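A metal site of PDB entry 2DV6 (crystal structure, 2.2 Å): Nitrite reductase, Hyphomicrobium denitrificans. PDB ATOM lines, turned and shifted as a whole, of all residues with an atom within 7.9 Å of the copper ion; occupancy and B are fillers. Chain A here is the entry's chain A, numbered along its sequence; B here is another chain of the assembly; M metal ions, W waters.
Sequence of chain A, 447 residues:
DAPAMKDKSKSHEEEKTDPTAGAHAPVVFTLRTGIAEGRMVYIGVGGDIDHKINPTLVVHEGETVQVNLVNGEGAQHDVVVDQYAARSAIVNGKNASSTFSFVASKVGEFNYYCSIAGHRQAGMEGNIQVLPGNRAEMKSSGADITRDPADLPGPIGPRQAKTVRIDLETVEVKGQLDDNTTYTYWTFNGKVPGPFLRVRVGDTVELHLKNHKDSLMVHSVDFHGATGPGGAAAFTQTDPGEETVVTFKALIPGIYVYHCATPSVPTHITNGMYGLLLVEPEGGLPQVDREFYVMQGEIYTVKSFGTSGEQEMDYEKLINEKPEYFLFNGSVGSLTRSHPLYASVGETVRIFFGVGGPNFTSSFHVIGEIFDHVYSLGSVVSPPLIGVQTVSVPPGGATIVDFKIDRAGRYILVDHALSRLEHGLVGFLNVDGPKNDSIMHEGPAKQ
The copper ion is bound by NE2 of His 259, NE2 of His 224, NE2 of His 416 of chain B and water W1.
The copper ion has four donor atoms within binding distance.
The backbone NH of His 365 of chain B is in hydrogen-bond range of the backbone carbonyl oxygen of Val 414 of chain B, 3.0 Å away.
OE1 of Gln 389 of chain B sits at hydrogen-bond distance from ND1 of His 224 (2.8 Å).
A ring nitrogen (NE2) of His 365 of chain B lies close to a ring nitrogen (NE2) of His 224, at 3.4 Å.
ND1 of His 365 of chain B lies within hydrogen-bond range of O of Gln 389 of chain B (2.5 Å).
A ring nitrogen (ND1) of His 224 lies close to the backbone carbonyl oxygen (O) of Gly 396, at 3.0 Å.
O of His 259 is in hydrogen-bond range of N of Asp 222, 2.8 Å away.
The backbone carbonyl oxygen (O) of Val 257 is in hydrogen-bond range of the backbone NH (N) of His 224, at 2.9 Å.
A ring nitrogen (ND1) of His 365 of chain B is in hydrogen-bond range of the side-chain hydroxyl (OG1) of Thr 390 of chain B (3.3 Å).
Residues that only touch the copper ion: Asp 222 and His 365 of chain B.
Within 4 Å of the copper ion: Asp 222, His 224, His 259, His 365 of chain B and His 416 of chain B.
The nearest printed residue that does not touch the copper ion is Leu 418 of chain B (4.9 Å).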
ATOM      1  N   ASP A 222       0.302  22.389   0.225  1.00  0.00           N
ATOM      2  CA  ASP A 222      -0.355  22.254  -1.089  1.00  0.00           C
ATOM      3  C   ASP A 222      -1.719  21.604  -0.745  1.00  0.00           C
ATOM      4  O   ASP A 222      -1.736  20.509  -0.176  1.00  0.00           O
ATOM      5  CB  ASP A 222       0.531  21.319  -1.961  1.00  0.00           C
ATOM      6  CG  ASP A 222      -0.151  20.794  -3.277  1.00  0.00           C
ATOM      7  OD1 ASP A 222       0.603  20.204  -4.111  1.00  0.00           O
ATOM      8  OD2 ASP A 222      -1.379  20.950  -3.516  1.00  0.00           O
ATOM      9  N   PHE A 223      -2.846  22.271  -1.048  1.00  0.00           N
ATOM     10  CA  PHE A 223      -4.190  21.675  -0.907  1.00  0.00           C
ATOM     11  C   PHE A 223      -4.692  21.168  -2.265  1.00  0.00           C
ATOM     12  O   PHE A 223      -4.745  21.954  -3.224  1.00  0.00           O
ATOM     13  CB  PHE A 223      -5.230  22.683  -0.369  1.00  0.00           C
ATOM     14  CG  PHE A 223      -4.882  23.314   0.967  1.00  0.00           C
ATOM     15  CD1 PHE A 223      -4.203  24.549   1.026  1.00  0.00           C
ATOM     16  CD2 PHE A 223      -5.257  22.707   2.149  1.00  0.00           C
ATOM     17  CE1 PHE A 223      -3.893  25.134   2.253  1.00  0.00           C
ATOM     18  CE2 PHE A 223      -4.957  23.278   3.377  1.00  0.00           C
ATOM     19  CZ  PHE A 223      -4.250  24.490   3.438  1.00  0.00           C
ATOM     20  N   HIS A 224      -5.093  19.894  -2.359  1.00  0.00           N
ATOM     21  CA  HIS A 224      -5.646  19.370  -3.636  1.00  0.00           C
ATOM     22  C   HIS A 224      -7.023  19.986  -3.962  1.00  0.00           C
ATOM     23  O   HIS A 224      -7.475  19.911  -5.109  1.00  0.00           O
ATOM     24  CB  HIS A 224      -5.757  17.834  -3.643  1.00  0.00           C
ATOM     25  CG  HIS A 224      -4.439  17.138  -3.693  1.00  0.00           C
ATOM     26  ND1 HIS A 224      -4.336  15.768  -3.827  1.00  0.00           N
ATOM     27  CD2 HIS A 224      -3.176  17.610  -3.674  1.00  0.00           C
ATOM     28  CE1 HIS A 224      -3.053  15.421  -3.843  1.00  0.00           C
ATOM     29  NE2 HIS A 224      -2.336  16.514  -3.753  1.00  0.00           N
ATOM     30  N   GLY A 230       0.991  25.630  -7.196  1.00  0.00           N
ATOM     31  CA  GLY A 230       1.362  24.700  -6.129  1.00  0.00           C
ATOM     32  C   GLY A 230       0.225  24.288  -5.192  1.00  0.00           C
ATOM     33  O   GLY A 230       0.471  23.808  -4.097  1.00  0.00           O
ATOM     34  N   VAL A 257      -6.708  15.540  -0.332  1.00  0.00           N
ATOM     35  CA  VAL A 257      -5.527  15.555   0.526  1.00  0.00           C
ATOM     36  C   VAL A 257      -4.816  16.886   0.457  1.00  0.00           C
ATOM     37  O   VAL A 257      -4.885  17.604  -0.551  1.00  0.00           O
ATOM     38  CB  VAL A 257      -4.600  14.262   0.455  1.00  0.00           C
ATOM     39  CG1 VAL A 257      -5.079  13.239  -0.538  1.00  0.00           C
ATOM     40  CG2 VAL A 257      -3.075  14.552   0.483  1.00  0.00           C
ATOM     41  N   TYR A 258      -4.159  17.241   1.565  1.00  0.00           N
ATOM     42  CA  TYR A 258      -3.205  18.332   1.504  1.00  0.00           C
ATOM     43  C   TYR A 258      -1.922  17.851   2.161  1.00  0.00           C
ATOM     44  O   TYR A 258      -1.971  16.928   2.964  1.00  0.00           O
ATOM     45  CB  TYR A 258      -3.760  19.590   2.193  1.00  0.00           C
ATOM     46  CG  TYR A 258      -3.878  19.517   3.695  1.00  0.00           C
ATOM     47  CD1 TYR A 258      -2.787  19.781   4.499  1.00  0.00           C
ATOM     48  CD2 TYR A 258      -5.102  19.221   4.310  1.00  0.00           C
ATOM     49  CE1 TYR A 258      -2.889  19.738   5.926  1.00  0.00           C
ATOM     50  CE2 TYR A 258      -5.217  19.188   5.703  1.00  0.00           C
ATOM     51  CZ  TYR A 258      -4.100  19.460   6.511  1.00  0.00           C
ATOM     52  OH  TYR A 258      -4.167  19.418   7.901  1.00  0.00           O
ATOM     53  N   HIS A 259      -0.799  18.473   1.843  1.00  0.00           N
ATOM     54  CA  HIS A 259       0.479  18.039   2.381  1.00  0.00           C
ATOM     55  C   HIS A 259       1.502  19.154   2.249  1.00  0.00           C
ATOM     56  O   HIS A 259       1.314  20.091   1.464  1.00  0.00           O
ATOM     57  CB  HIS A 259       0.956  16.775   1.620  1.00  0.00           C
ATOM     58  CG  HIS A 259       0.955  16.937   0.138  1.00  0.00           C
ATOM     59  ND1 HIS A 259       1.971  17.586  -0.542  1.00  0.00           N
ATOM     60  CD2 HIS A 259       0.063  16.547  -0.803  1.00  0.00           C
ATOM     61  CE1 HIS A 259       1.714  17.573  -1.838  1.00  0.00           C
ATOM     62  NE2 HIS A 259       0.555  16.954  -2.023  1.00  0.00           N
ATOM     63  N   CYS A 260       2.596  19.065   2.992  1.00  0.00           N
ATOM     64  CA  CYS A 260       3.681  20.010   2.784  1.00  0.00           C
ATOM     65  C   CYS A 260       4.192  19.857   1.360  1.00  0.00           C
ATOM     66  O   CYS A 260       4.196  18.764   0.793  1.00  0.00           O
ATOM     67  CB  CYS A 260       4.802  19.764   3.779  1.00  0.00           C
ATOM     68  SG  CYS A 260       6.201  20.911   3.669  1.00  0.00           S
ATOM     69  N   ALA A 261       4.597  20.979   0.780  1.00  0.00           N
ATOM     70  CA  ALA A 261       5.118  20.982  -0.575  1.00  0.00           C
ATOM     71  C   ALA A 261       6.501  21.644  -0.654  1.00  0.00           C
ATOM     72  O   ALA A 261       6.824  22.312  -1.645  1.00  0.00           O
ATOM     73  CB  ALA A 261       4.118  21.658  -1.549  1.00  0.00           C
ATOM     74  N   VAL A 265       9.727  16.921  -1.328  1.00  0.00           N
ATOM     75  CA  VAL A 265       8.332  16.705  -0.950  1.00  0.00           C
ATOM     76  C   VAL A 265       8.075  15.307  -0.359  1.00  0.00           C
ATOM     77  O   VAL A 265       7.467  15.235   0.699  1.00  0.00           O
ATOM     78  CB  VAL A 265       7.311  17.031  -2.086  1.00  0.00           C
ATOM     79  CG1 VAL A 265       5.892  16.808  -1.572  1.00  0.00           C
ATOM     80  CG2 VAL A 265       7.457  18.514  -2.545  1.00  0.00           C
ATOM     81  N   ILE A 269       6.420  14.557   3.394  1.00  0.00           N
ATOM     82  CA  ILE A 269       5.237  13.689   3.497  1.00  0.00           C
ATOM     83  C   ILE A 269       5.513  12.460   4.342  1.00  0.00           C
ATOM     84  O   ILE A 269       4.776  12.186   5.316  1.00  0.00           O
ATOM     85  CB  ILE A 269       4.699  13.285   2.121  1.00  0.00           C
ATOM     86  CG1 ILE A 269       4.050  14.486   1.458  1.00  0.00           C
ATOM     87  CG2 ILE A 269       3.664  12.120   2.231  1.00  0.00           C
ATOM     88  CD1 ILE A 269       3.741  14.236  -0.025  1.00  0.00           C
ATOM     89  N   GLY A 356      -1.694   9.723   2.514  1.00  0.00           N
ATOM     90  CA  GLY A 356      -0.543  10.632   2.443  1.00  0.00           C
ATOM     91  C   GLY A 356       0.568   9.961   1.626  1.00  0.00           C
ATOM     92  O   GLY A 356       1.145  10.575   0.751  1.00  0.00           O
ATOM     93  N   PRO A 395      -1.823   7.249  -3.423  1.00  0.00           N
ATOM     94  CA  PRO A 395      -1.202   8.301  -2.606  1.00  0.00           C
ATOM     95  C   PRO A 395      -1.625   9.640  -3.214  1.00  0.00           C
ATOM     96  O   PRO A 395      -1.760   9.723  -4.416  1.00  0.00           O
ATOM     97  CB  PRO A 395       0.279   8.021  -2.749  1.00  0.00           C
ATOM     98  CG  PRO A 395       0.411   7.173  -4.073  1.00  0.00           C
ATOM     99  CD  PRO A 395      -0.853   6.412  -4.151  1.00  0.00           C
ATOM    100  N   GLY A 396      -1.906  10.627  -2.360  1.00  0.00           N
ATOM    101  CA  GLY A 396      -2.415  11.905  -2.805  1.00  0.00           C
ATOM    102  C   GLY A 396      -3.860  11.839  -3.251  1.00  0.00           C
ATOM    103  O   GLY A 396      -4.335  12.741  -3.990  1.00  0.00           O
ATOM    104  N   GLY A 397      -4.561  10.797  -2.808  1.00  0.00           N
ATOM    105  CA  GLY A 397      -5.970  10.630  -3.083  1.00  0.00           C
ATOM    106  C   GLY A 397      -6.707  10.304  -1.779  1.00  0.00           C
ATOM    107  O   GLY A 397      -6.082   9.924  -0.782  1.00  0.00           O
ATOM    108  N   HIS B 365      -1.898  13.221 -11.265  1.00  0.00           N
ATOM    109  CA  HIS B 365      -2.403  14.380 -10.557  1.00  0.00           C
ATOM    110  C   HIS B 365      -1.793  15.618 -11.198  1.00  0.00           C
ATOM    111  O   HIS B 365      -0.632  15.583 -11.606  1.00  0.00           O
ATOM    112  CB  HIS B 365      -1.961  14.269  -9.094  1.00  0.00           C
ATOM    113  CG  HIS B 365      -2.311  15.453  -8.273  1.00  0.00           C
ATOM    114  ND1 HIS B 365      -3.617  15.796  -7.969  1.00  0.00           N
ATOM    115  CD2 HIS B 365      -1.536  16.420  -7.733  1.00  0.00           C
ATOM    116  CE1 HIS B 365      -3.616  16.908  -7.273  1.00  0.00           C
ATOM    117  NE2 HIS B 365      -2.372  17.302  -7.105  1.00  0.00           N
ATOM    118  N   VAL B 366      -2.550  16.710 -11.279  1.00  0.00           N
ATOM    119  CA  VAL B 366      -2.011  18.009 -11.755  1.00  0.00           C
ATOM    120  C   VAL B 366      -2.007  18.997 -10.583  1.00  0.00           C
ATOM    121  O   VAL B 366      -3.066  19.475 -10.161  1.00  0.00           O
ATOM    122  CB  VAL B 366      -2.789  18.573 -13.017  1.00  0.00           C
ATOM    123  CG1 VAL B 366      -2.267  19.961 -13.454  1.00  0.00           C
ATOM    124  CG2 VAL B 366      -2.717  17.592 -14.205  1.00  0.00           C
ATOM    125  N   ILE B 367      -0.826  19.272 -10.027  1.00  0.00           N
ATOM    126  CA  ILE B 367      -0.691  20.138  -8.845  1.00  0.00           C
ATOM    127  C   ILE B 367      -1.216  21.536  -9.162  1.00  0.00           C
ATOM    128  O   ILE B 367      -0.784  22.176 -10.127  1.00  0.00           O
ATOM    129  CB  ILE B 367       0.806  20.273  -8.438  1.00  0.00           C
ATOM    130  CG1 ILE B 367       1.418  18.918  -8.032  1.00  0.00           C
ATOM    131  CG2 ILE B 367       1.001  21.350  -7.334  1.00  0.00           C
ATOM    132  CD1 ILE B 367       2.937  18.950  -7.829  1.00  0.00           C
ATOM    133  N   GLY B 368      -2.157  22.009  -8.343  1.00  0.00           N
ATOM    134  CA  GLY B 368      -2.750  23.324  -8.526  1.00  0.00           C
ATOM    135  C   GLY B 368      -4.051  23.297  -9.295  1.00  0.00           C
ATOM    136  O   GLY B 368      -4.713  24.312  -9.410  1.00  0.00           O
ATOM    137  N   GLN B 389      -9.301  14.732  -7.638  1.00  0.00           N
ATOM    138  CA  GLN B 389      -7.930  15.260  -7.498  1.00  0.00           C
ATOM    139  C   GLN B 389      -6.864  14.420  -8.214  1.00  0.00           C
ATOM    140  O   GLN B 389      -5.876  14.969  -8.743  1.00  0.00           O
ATOM    141  CB  GLN B 389      -7.537  15.434  -6.030  1.00  0.00           C
ATOM    142  CG  GLN B 389      -7.395  14.073  -5.282  1.00  0.00           C
ATOM    143  CD  GLN B 389      -7.641  14.215  -3.805  1.00  0.00           C
ATOM    144  OE1 GLN B 389      -6.815  14.810  -3.095  1.00  0.00           O
ATOM    145  NE2 GLN B 389      -8.758  13.621  -3.322  1.00  0.00           N
ATOM    146  N   THR B 390      -7.028  13.090  -8.180  1.00  0.00           N
ATOM    147  CA  THR B 390      -5.941  12.160  -8.525  1.00  0.00           C
ATOM    148  C   THR B 390      -6.567  10.937  -9.153  1.00  0.00           C
ATOM    149  O   THR B 390      -7.577  10.465  -8.678  1.00  0.00           O
ATOM    150  CB  THR B 390      -5.169  11.734  -7.252  1.00  0.00           C
ATOM    151  OG1 THR B 390      -4.574  12.892  -6.640  1.00  0.00           O
ATOM    152  CG2 THR B 390      -4.066  10.613  -7.568  1.00  0.00           C
ATOM    153  N   VAL B 414       2.283  15.054 -12.258  1.00  0.00           N
ATOM    154  CA  VAL B 414       3.041  14.119 -11.394  1.00  0.00           C
ATOM    155  C   VAL B 414       2.287  12.792 -11.298  1.00  0.00           C
ATOM    156  O   VAL B 414       1.072  12.730 -11.533  1.00  0.00           O
ATOM    157  CB  VAL B 414       3.223  14.642  -9.910  1.00  0.00           C
ATOM    158  CG1 VAL B 414       4.007  15.955  -9.867  1.00  0.00           C
ATOM    159  CG2 VAL B 414       1.853  14.778  -9.180  1.00  0.00           C
ATOM    160  N   HIS B 416       1.472  10.853  -8.176  1.00  0.00           N
ATOM    161  CA  HIS B 416       1.555  11.210  -6.748  1.00  0.00           C
ATOM    162  C   HIS B 416       2.199  10.175  -5.815  1.00  0.00           C
ATOM    163  O   HIS B 416       2.191  10.350  -4.569  1.00  0.00           O
ATOM    164  CB  HIS B 416       0.178  11.630  -6.207  1.00  0.00           C
ATOM    165  CG  HIS B 416       0.252  12.728  -5.195  1.00  0.00           C
ATOM    166  ND1 HIS B 416       0.752  12.537  -3.920  1.00  0.00           N
ATOM    167  CD2 HIS B 416      -0.106  14.033  -5.281  1.00  0.00           C
ATOM    168  CE1 HIS B 416       0.703  13.682  -3.254  1.00  0.00           C
ATOM    169  NE2 HIS B 416       0.201  14.605  -4.059  1.00  0.00           N
ATOM    170  N   LEU B 418       5.247  10.035  -4.815  1.00  0.00           N
ATOM    171  CA  LEU B 418       6.089  11.220  -5.031  1.00  0.00           C
ATOM    172  C   LEU B 418       7.604  10.978  -4.955  1.00  0.00           C
ATOM    173  O   LEU B 418       8.385  11.837  -5.366  1.00  0.00           O
ATOM    174  CB  LEU B 418       5.637  12.341  -4.087  1.00  0.00           C
ATOM    175  CG  LEU B 418       4.836  13.557  -4.599  1.00  0.00           C
ATOM    176  CD1 LEU B 418       4.330  13.571  -6.042  1.00  0.00           C
ATOM    177  CD2 LEU B 418       3.807  13.986  -3.636  1.00  0.00           C
HETATM  178 CU    CU M   1      -0.258  16.636  -3.860  1.00  0.00          CU
HETATM  179  O   HOH W   1       1.543  17.523  -5.404  1.00  0.00           O
